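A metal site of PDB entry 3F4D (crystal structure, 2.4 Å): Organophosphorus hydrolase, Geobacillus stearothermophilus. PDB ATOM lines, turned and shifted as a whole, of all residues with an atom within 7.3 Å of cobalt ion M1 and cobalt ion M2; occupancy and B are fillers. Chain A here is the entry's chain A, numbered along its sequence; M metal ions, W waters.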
ATOM      1  N   HIS A  23      16.451  29.614   3.710  1.00  0.00           N
ATOM      2  CA  HIS A  23      16.577  28.770   4.883  1.00  0.00           C
ATOM      3  C   HIS A  23      15.333  28.761   5.731  1.00  0.00           C
ATOM      4  O   HIS A  23      15.103  29.690   6.509  1.00  0.00           O
ATOM      5  CB  HIS A  23      17.787  29.246   5.730  1.00  0.00           C
ATOM      6  CG  HIS A  23      18.185  28.296   6.824  1.00  0.00           C
ATOM      7  ND1 HIS A  23      19.499  28.038   7.138  1.00  0.00           N
ATOM      8  CD2 HIS A  23      17.448  27.589   7.727  1.00  0.00           C
ATOM      9  CE1 HIS A  23      19.570  27.211   8.166  1.00  0.00           C
ATOM     10  NE2 HIS A  23      18.338  26.931   8.546  1.00  0.00           N
ATOM     11  N   GLU A  24      14.536  27.705   5.562  1.00  0.00           N
ATOM     12  CA  GLU A  24      13.299  27.484   6.293  1.00  0.00           C
ATOM     13  C   GLU A  24      13.125  25.960   6.519  1.00  0.00           C
ATOM     14  O   GLU A  24      13.570  25.139   5.724  1.00  0.00           O
ATOM     15  CB  GLU A  24      12.084  28.006   5.522  1.00  0.00           C
ATOM     16  CG  GLU A  24      12.126  29.498   5.123  1.00  0.00           C
ATOM     17  CD  GLU A  24      12.148  30.470   6.309  1.00  0.00           C
ATOM     18  OE1 GLU A  24      11.765  30.108   7.443  1.00  0.00           O
ATOM     19  OE2 GLU A  24      12.539  31.628   6.103  1.00  0.00           O
ATOM     20  N   HIS A  25      12.471  25.594   7.626  1.00  0.00           N
ATOM     21  CA  HIS A  25      12.248  24.195   7.954  1.00  0.00           C
ATOM     22  C   HIS A  25      10.765  23.872   8.019  1.00  0.00           C
ATOM     23  O   HIS A  25      10.047  24.441   8.841  1.00  0.00           O
ATOM     24  CB  HIS A  25      12.844  23.844   9.326  1.00  0.00           C
ATOM     25  CG  HIS A  25      14.320  24.048   9.431  1.00  0.00           C
ATOM     26  ND1 HIS A  25      15.238  23.099   9.039  1.00  0.00           N
ATOM     27  CD2 HIS A  25      15.040  25.114   9.860  1.00  0.00           C
ATOM     28  CE1 HIS A  25      16.461  23.579   9.208  1.00  0.00           C
ATOM     29  NE2 HIS A  25      16.359  24.796   9.712  1.00  0.00           N
ATOM     30  N   PHE A  28      11.037  19.829  11.871  1.00  0.00           N
ATOM     31  CA  PHE A  28      12.296  19.851  12.560  1.00  0.00           C
ATOM     32  C   PHE A  28      12.220  19.221  13.932  1.00  0.00           C
ATOM     33  O   PHE A  28      11.230  19.390  14.671  1.00  0.00           O
ATOM     34  CB  PHE A  28      12.853  21.271  12.656  1.00  0.00           C
ATOM     35  CG  PHE A  28      14.234  21.315  13.239  1.00  0.00           C
ATOM     36  CD1 PHE A  28      14.432  21.186  14.622  1.00  0.00           C
ATOM     37  CD2 PHE A  28      15.360  21.377  12.411  1.00  0.00           C
ATOM     38  CE1 PHE A  28      15.690  21.114  15.170  1.00  0.00           C
ATOM     39  CE2 PHE A  28      16.632  21.303  12.942  1.00  0.00           C
ATOM     40  CZ  PHE A  28      16.799  21.165  14.330  1.00  0.00           C
ATOM     41  N   PRO A  69      16.931  23.174   4.630  1.00  0.00           N
ATOM     42  CA  PRO A  69      18.182  22.481   4.965  1.00  0.00           C
ATOM     43  C   PRO A  69      18.193  21.613   6.215  1.00  0.00           C
ATOM     44  O   PRO A  69      19.230  21.470   6.847  1.00  0.00           O
ATOM     45  CB  PRO A  69      19.165  23.647   5.094  1.00  0.00           C
ATOM     46  CG  PRO A  69      18.312  24.646   5.862  1.00  0.00           C
ATOM     47  CD  PRO A  69      16.879  24.507   5.265  1.00  0.00           C
ATOM     48  N   THR A  70      17.045  21.048   6.573  1.00  0.00           N
ATOM     49  CA  THR A  70      16.937  20.173   7.739  1.00  0.00           C
ATOM     50  C   THR A  70      17.919  19.005   7.661  1.00  0.00           C
ATOM     51  O   THR A  70      17.850  18.167   6.751  1.00  0.00           O
ATOM     52  CB  THR A  70      15.513  19.611   7.878  1.00  0.00           C
ATOM     53  OG1 THR A  70      14.581  20.686   8.020  1.00  0.00           O
ATOM     54  CG2 THR A  70      15.420  18.706   9.106  1.00  0.00           C
ATOM     55  N   PRO A  71      18.836  18.904   8.635  1.00  0.00           N
ATOM     56  CA  PRO A  71      19.862  17.854   8.717  1.00  0.00           C
ATOM     57  C   PRO A  71      19.333  16.401   8.775  1.00  0.00           C
ATOM     58  O   PRO A  71      18.241  16.155   9.247  1.00  0.00           O
ATOM     59  CB  PRO A  71      20.626  18.226   9.983  1.00  0.00           C
ATOM     60  CG  PRO A  71      20.463  19.740  10.052  1.00  0.00           C
ATOM     61  CD  PRO A  71      18.994  19.895   9.715  1.00  0.00           C
ATOM     62  N   TYR A  99      23.848  17.687  11.835  1.00  0.00           N
ATOM     63  CA  TYR A  99      23.913  18.901  12.636  1.00  0.00           C
ATOM     64  C   TYR A  99      25.290  19.045  13.337  1.00  0.00           C
ATOM     65  O   TYR A  99      26.105  18.118  13.322  1.00  0.00           O
ATOM     66  CB  TYR A  99      22.785  18.919  13.668  1.00  0.00           C
ATOM     67  CG  TYR A  99      22.223  20.311  13.882  1.00  0.00           C
ATOM     68  CD1 TYR A  99      22.348  21.288  12.903  1.00  0.00           C
ATOM     69  CD2 TYR A  99      21.529  20.645  15.062  1.00  0.00           C
ATOM     70  CE1 TYR A  99      21.813  22.552  13.055  1.00  0.00           C
ATOM     71  CE2 TYR A  99      20.983  21.927  15.227  1.00  0.00           C
ATOM     72  CZ  TYR A  99      21.131  22.876  14.212  1.00  0.00           C
ATOM     73  OH  TYR A  99      20.598  24.151  14.336  1.00  0.00           O
ATOM     74  N   TYR A 100      25.539  20.211  13.923  1.00  0.00           N
ATOM     75  CA  TYR A 100      26.806  20.414  14.604  1.00  0.00           C
ATOM     76  C   TYR A 100      26.897  19.517  15.848  1.00  0.00           C
ATOM     77  O   TYR A 100      25.893  19.035  16.365  1.00  0.00           O
ATOM     78  CB  TYR A 100      26.996  21.906  14.955  1.00  0.00           C
ATOM     79  CG  TYR A 100      26.128  22.453  16.063  1.00  0.00           C
ATOM     80  CD1 TYR A 100      24.753  22.548  15.908  1.00  0.00           C
ATOM     81  CD2 TYR A 100      26.695  22.883  17.254  1.00  0.00           C
ATOM     82  CE1 TYR A 100      23.950  23.061  16.927  1.00  0.00           C
ATOM     83  CE2 TYR A 100      25.911  23.387  18.279  1.00  0.00           C
ATOM     84  CZ  TYR A 100      24.543  23.477  18.113  1.00  0.00           C
ATOM     85  OH  TYR A 100      23.763  23.968  19.136  1.00  0.00           O
ATOM     86  N   KCX A 145      24.454  20.368   3.664  1.00  0.00           N
ATOM     87  CA  KCX A 145      24.288  21.167   4.856  1.00  0.00           C
ATOM     88  CB  KCX A 145      22.940  20.852   5.526  1.00  0.00           C
ATOM     89  CG  KCX A 145      22.746  21.564   6.873  1.00  0.00           C
ATOM     90  CD  KCX A 145      22.876  23.057   6.695  1.00  0.00           C
ATOM     91  CE  KCX A 145      22.668  23.799   7.980  1.00  0.00           C
ATOM     92  NZ  KCX A 145      21.310  23.597   8.492  1.00  0.00           N
ATOM     93  C   KCX A 145      25.435  20.932   5.858  1.00  0.00           C
ATOM     94  O   KCX A 145      25.690  19.793   6.262  1.00  0.00           O
ATOM     95  CX  KCX A 145      20.774  24.310   9.468  1.00  0.00           C
ATOM     96  OQ1 KCX A 145      19.601  24.089   9.870  1.00  0.00           O
ATOM     97  OQ2 KCX A 145      21.398  25.283   9.969  1.00  0.00           O
ATOM     98  N   LEU A 146      26.098  22.005   6.264  1.00  0.00           N
ATOM     99  CA  LEU A 146      27.184  21.910   7.230  1.00  0.00           C
ATOM    100  C   LEU A 146      26.910  22.801   8.439  1.00  0.00           C
ATOM    101  O   LEU A 146      26.155  23.769   8.343  1.00  0.00           O
ATOM    102  CB  LEU A 146      28.500  22.360   6.599  1.00  0.00           C
ATOM    103  CG  LEU A 146      29.183  21.505   5.527  1.00  0.00           C
ATOM    104  CD1 LEU A 146      30.409  22.303   5.033  1.00  0.00           C
ATOM    105  CD2 LEU A 146      29.589  20.117   6.099  1.00  0.00           C
ATOM    106  N   ALA A 147      27.561  22.501   9.550  1.00  0.00           N
ATOM    107  CA  ALA A 147      27.400  23.290  10.782  1.00  0.00           C
ATOM    108  C   ALA A 147      28.626  23.204  11.699  1.00  0.00           C
ATOM    109  O   ALA A 147      29.305  22.194  11.756  1.00  0.00           O
ATOM    110  CB  ALA A 147      26.153  22.823  11.522  1.00  0.00           C
ATOM    111  N   THR A 177      25.736  26.628   5.204  1.00  0.00           N
ATOM    112  CA  THR A 177      26.223  26.402   6.555  1.00  0.00           C
ATOM    113  C   THR A 177      25.465  27.068   7.680  1.00  0.00           C
ATOM    114  O   THR A 177      24.722  28.025   7.485  1.00  0.00           O
ATOM    115  CB  THR A 177      27.694  26.821   6.724  1.00  0.00           C
ATOM    116  OG1 THR A 177      27.753  28.223   6.984  1.00  0.00           O
ATOM    117  CG2 THR A 177      28.483  26.521   5.478  1.00  0.00           C
ATOM    118  N   HIS A 178      25.701  26.529   8.874  1.00  0.00           N
ATOM    119  CA  HIS A 178      25.122  27.003  10.108  1.00  0.00           C
ATOM    120  C   HIS A 178      26.294  27.413  10.995  1.00  0.00           C
ATOM    121  O   HIS A 178      27.219  26.634  11.196  1.00  0.00           O
ATOM    122  CB  HIS A 178      24.343  25.827  10.787  1.00  0.00           C
ATOM    123  CG  HIS A 178      24.192  25.965  12.273  1.00  0.00           C
ATOM    124  ND1 HIS A 178      22.963  25.993  12.886  1.00  0.00           N
ATOM    125  CD2 HIS A 178      25.104  26.054  13.263  1.00  0.00           C
ATOM    126  CE1 HIS A 178      23.125  26.103  14.190  1.00  0.00           C
ATOM    127  NE2 HIS A 178      24.417  26.146  14.441  1.00  0.00           N
ATOM    128  N   THR A 179      26.298  28.648  11.478  1.00  0.00           N
ATOM    129  CA  THR A 179      27.326  29.093  12.412  1.00  0.00           C
ATOM    130  C   THR A 179      26.582  29.275  13.736  1.00  0.00           C
ATOM    131  O   THR A 179      25.401  29.657  13.770  1.00  0.00           O
ATOM    132  CB  THR A 179      27.974  30.443  12.035  1.00  0.00           C
ATOM    133  OG1 THR A 179      26.955  31.428  11.855  1.00  0.00           O
ATOM    134  CG2 THR A 179      28.847  30.309  10.776  1.00  0.00           C
ATOM    135  N   GLN A 180      27.274  28.996  14.825  1.00  0.00           N
ATOM    136  CA  GLN A 180      26.684  29.039  16.157  1.00  0.00           C
ATOM    137  C   GLN A 180      27.023  30.329  16.917  1.00  0.00           C
ATOM    138  O   GLN A 180      28.194  30.624  17.175  1.00  0.00           O
ATOM    139  CB  GLN A 180      27.167  27.785  16.909  1.00  0.00           C
ATOM    140  CG  GLN A 180      26.493  27.450  18.220  1.00  0.00           C
ATOM    141  CD  GLN A 180      25.017  27.248  18.080  1.00  0.00           C
ATOM    142  OE1 GLN A 180      24.534  26.922  17.009  1.00  0.00           O
ATOM    143  NE2 GLN A 180      24.296  27.440  19.167  1.00  0.00           N
ATOM    144  N   GLY A 205      25.784  30.514   6.761  1.00  0.00           N
ATOM    145  CA  GLY A 205      24.550  30.936   7.418  1.00  0.00           C
ATOM    146  C   GLY A 205      24.645  31.545   8.802  1.00  0.00           C
ATOM    147  O   GLY A 205      25.725  31.549   9.423  1.00  0.00           O
ATOM    148  N   HIS A 206      23.503  32.053   9.270  1.00  0.00           N
ATOM    149  CA  HIS A 206      23.364  32.687  10.582  1.00  0.00           C
ATOM    150  C   HIS A 206      24.376  33.793  10.834  1.00  0.00           C
ATOM    151  O   HIS A 206      24.756  34.053  11.980  1.00  0.00           O
ATOM    152  CB  HIS A 206      23.457  31.653  11.705  1.00  0.00           C
ATOM    153  CG  HIS A 206      22.516  30.509  11.538  1.00  0.00           C
ATOM    154  ND1 HIS A 206      21.622  30.438  10.492  1.00  0.00           N
ATOM    155  CD2 HIS A 206      22.376  29.359  12.224  1.00  0.00           C
ATOM    156  CE1 HIS A 206      20.977  29.284  10.531  1.00  0.00           C
ATOM    157  NE2 HIS A 206      21.420  28.610  11.573  1.00  0.00           N
ATOM    158  N   ASP A 229      19.666  34.867   8.057  1.00  0.00           N
ATOM    159  CA  ASP A 229      18.551  33.938   8.003  1.00  0.00           C
ATOM    160  C   ASP A 229      17.799  33.641   9.275  1.00  0.00           C
ATOM    161  O   ASP A 229      17.104  32.641   9.338  1.00  0.00           O
ATOM    162  CB  ASP A 229      19.034  32.610   7.410  1.00  0.00           C
ATOM    163  CG  ASP A 229      20.229  32.070   8.145  1.00  0.00           C
ATOM    164  OD1 ASP A 229      20.357  32.370   9.348  1.00  0.00           O
ATOM    165  OD2 ASP A 229      21.040  31.344   7.526  1.00  0.00           O
ATOM    166  N   ARG A 230      17.928  34.489  10.279  1.00  0.00           N
ATOM    167  CA  ARG A 230      17.185  34.229  11.491  1.00  0.00           C
ATOM    168  C   ARG A 230      16.274  35.386  11.906  1.00  0.00           C
ATOM    169  O   ARG A 230      15.969  35.553  13.091  1.00  0.00           O
ATOM    170  CB  ARG A 230      18.144  33.820  12.609  1.00  0.00           C
ATOM    171  CG  ARG A 230      18.760  32.439  12.351  1.00  0.00           C
ATOM    172  CD  ARG A 230      19.893  32.146  13.284  1.00  0.00           C
ATOM    173  NE  ARG A 230      19.410  31.792  14.609  1.00  0.00           N
ATOM    174  CZ  ARG A 230      19.088  30.554  14.966  1.00  0.00           C
ATOM    175  NH1 ARG A 230      19.216  29.566  14.082  1.00  0.00           N
ATOM    176  NH2 ARG A 230      18.638  30.306  16.190  1.00  0.00           N
ATOM    177  N   ASP A 266      14.413  31.069   9.014  1.00  0.00           N
ATOM    178  CA  ASP A 266      14.837  29.843   9.675  1.00  0.00           C
ATOM    179  C   ASP A 266      13.696  29.241  10.539  1.00  0.00           C
ATOM    180  O   ASP A 266      13.940  28.585  11.556  1.00  0.00           O
ATOM    181  CB  ASP A 266      16.091  30.080  10.520  1.00  0.00           C
ATOM    182  CG  ASP A 266      16.714  28.776  11.027  1.00  0.00           C
ATOM    183  OD1 ASP A 266      16.309  27.688  10.549  1.00  0.00           O
ATOM    184  OD2 ASP A 266      17.623  28.851  11.894  1.00  0.00           O
ATOM    185  N   THR A 267      12.440  29.437  10.111  1.00  0.00           N
ATOM    186  CA  THR A 267      11.326  28.890  10.859  1.00  0.00           C
ATOM    187  C   THR A 267      11.317  27.357  10.954  1.00  0.00           C
ATOM    188  O   THR A 267      11.964  26.646  10.177  1.00  0.00           O
ATOM    189  CB  THR A 267       9.945  29.290  10.260  1.00  0.00           C
ATOM    190  OG1 THR A 267       9.834  28.792   8.908  1.00  0.00           O
ATOM    191  CG2 THR A 267       9.750  30.820  10.289  1.00  0.00           C
ATOM    192  N   VAL A 268      10.565  26.883  11.934  1.00  0.00           N
ATOM    193  CA  VAL A 268      10.360  25.473  12.192  1.00  0.00           C
ATOM    194  C   VAL A 268       8.853  25.442  12.222  1.00  0.00           C
ATOM    195  O   VAL A 268       8.233  25.780  13.236  1.00  0.00           O
ATOM    196  CB  VAL A 268      10.875  25.030  13.584  1.00  0.00           C
ATOM    197  CG1 VAL A 268      10.469  23.597  13.849  1.00  0.00           C
ATOM    198  CG2 VAL A 268      12.363  25.161  13.631  1.00  0.00           C
HETATM  199 CO    CO M   1      17.993  25.910  10.322  1.00  0.00          CO
HETATM  200 CO    CO M   2      20.872  26.352  11.930  1.00  0.00          CO
HETATM  201  O   HOH W   1      18.854  26.855  11.908  1.00  0.00           O
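The backbone NH (N) of His 25 is in hydrogen-bond range of the backbone carbonyl oxygen (O) of Thr 267 (2.8 Å). NZ of KCX 145 is in hydrogen-bond range of the backbone carbonyl oxygen (O) of Pro 69 (3.4 Å). OE1 of Gln 180 sits at hydrogen-bond distance from NE2 of His 178, at 2.7 Å. O of Leu 146 sits at hydrogen-bond distance from N of His 178, 2.8 Å away. A ring nitrogen (NE2) of His 206 sits close to the guanidinium group (NH1) of Arg 230, at 3.5 Å. O of His 206 is in hydrogen-bond range of OG1 of Thr 179. A ring nitrogen (ND1) of His 206 is in hydrogen-bond range of the side-chain carboxylate of Asp 229. The backbone NH (N) of Asp 266 is in hydrogen-bond range of the side-chain carboxylate (OE1) of Glu 24, at 3.2 Å.
Of the 23 residues printed, 4 come within 4 Å of cobalt ion M1. Along chain A the residues within 4 Å of cobalt ion M1 span positions 23 to 266. The nearest printed residue that does not touch cobalt ion M1 is His 206 (4.5 Å).
Tyr 99 touches cobalt ion M2. Four residues have an atom within 4 Å of cobalt ion M2: Tyr 99, KCX 145, His 178 and His 206. The nearest printed residue that does not touch cobalt ion M2 is His 23 (4.1 Å).
Water W1 is bound to cobalt ion M1 (2.0 Å). NE2 of His 25 binds cobalt ion M1 (2.1 Å). NE2 of His 23 binds cobalt ion M1 (2.1 Å). OD1 of Asp 266 is bound to cobalt ion M1 (2.5 Å). OQ1 of KCX 145 binds cobalt ion M1, 2.5 Å away. Cobalt ion M1 has five donor atoms within binding distance.
Cobalt ion M2 is bound by water W1 (2.1 Å), OQ2 of KCX 145 (2.3 Å), a ring nitrogen (ND1) of His 178 (2.3 Å) and a ring nitrogen (NE2) of His 206 (2.4 Å). Cobalt ion M2 has four donor atoms within binding distance.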
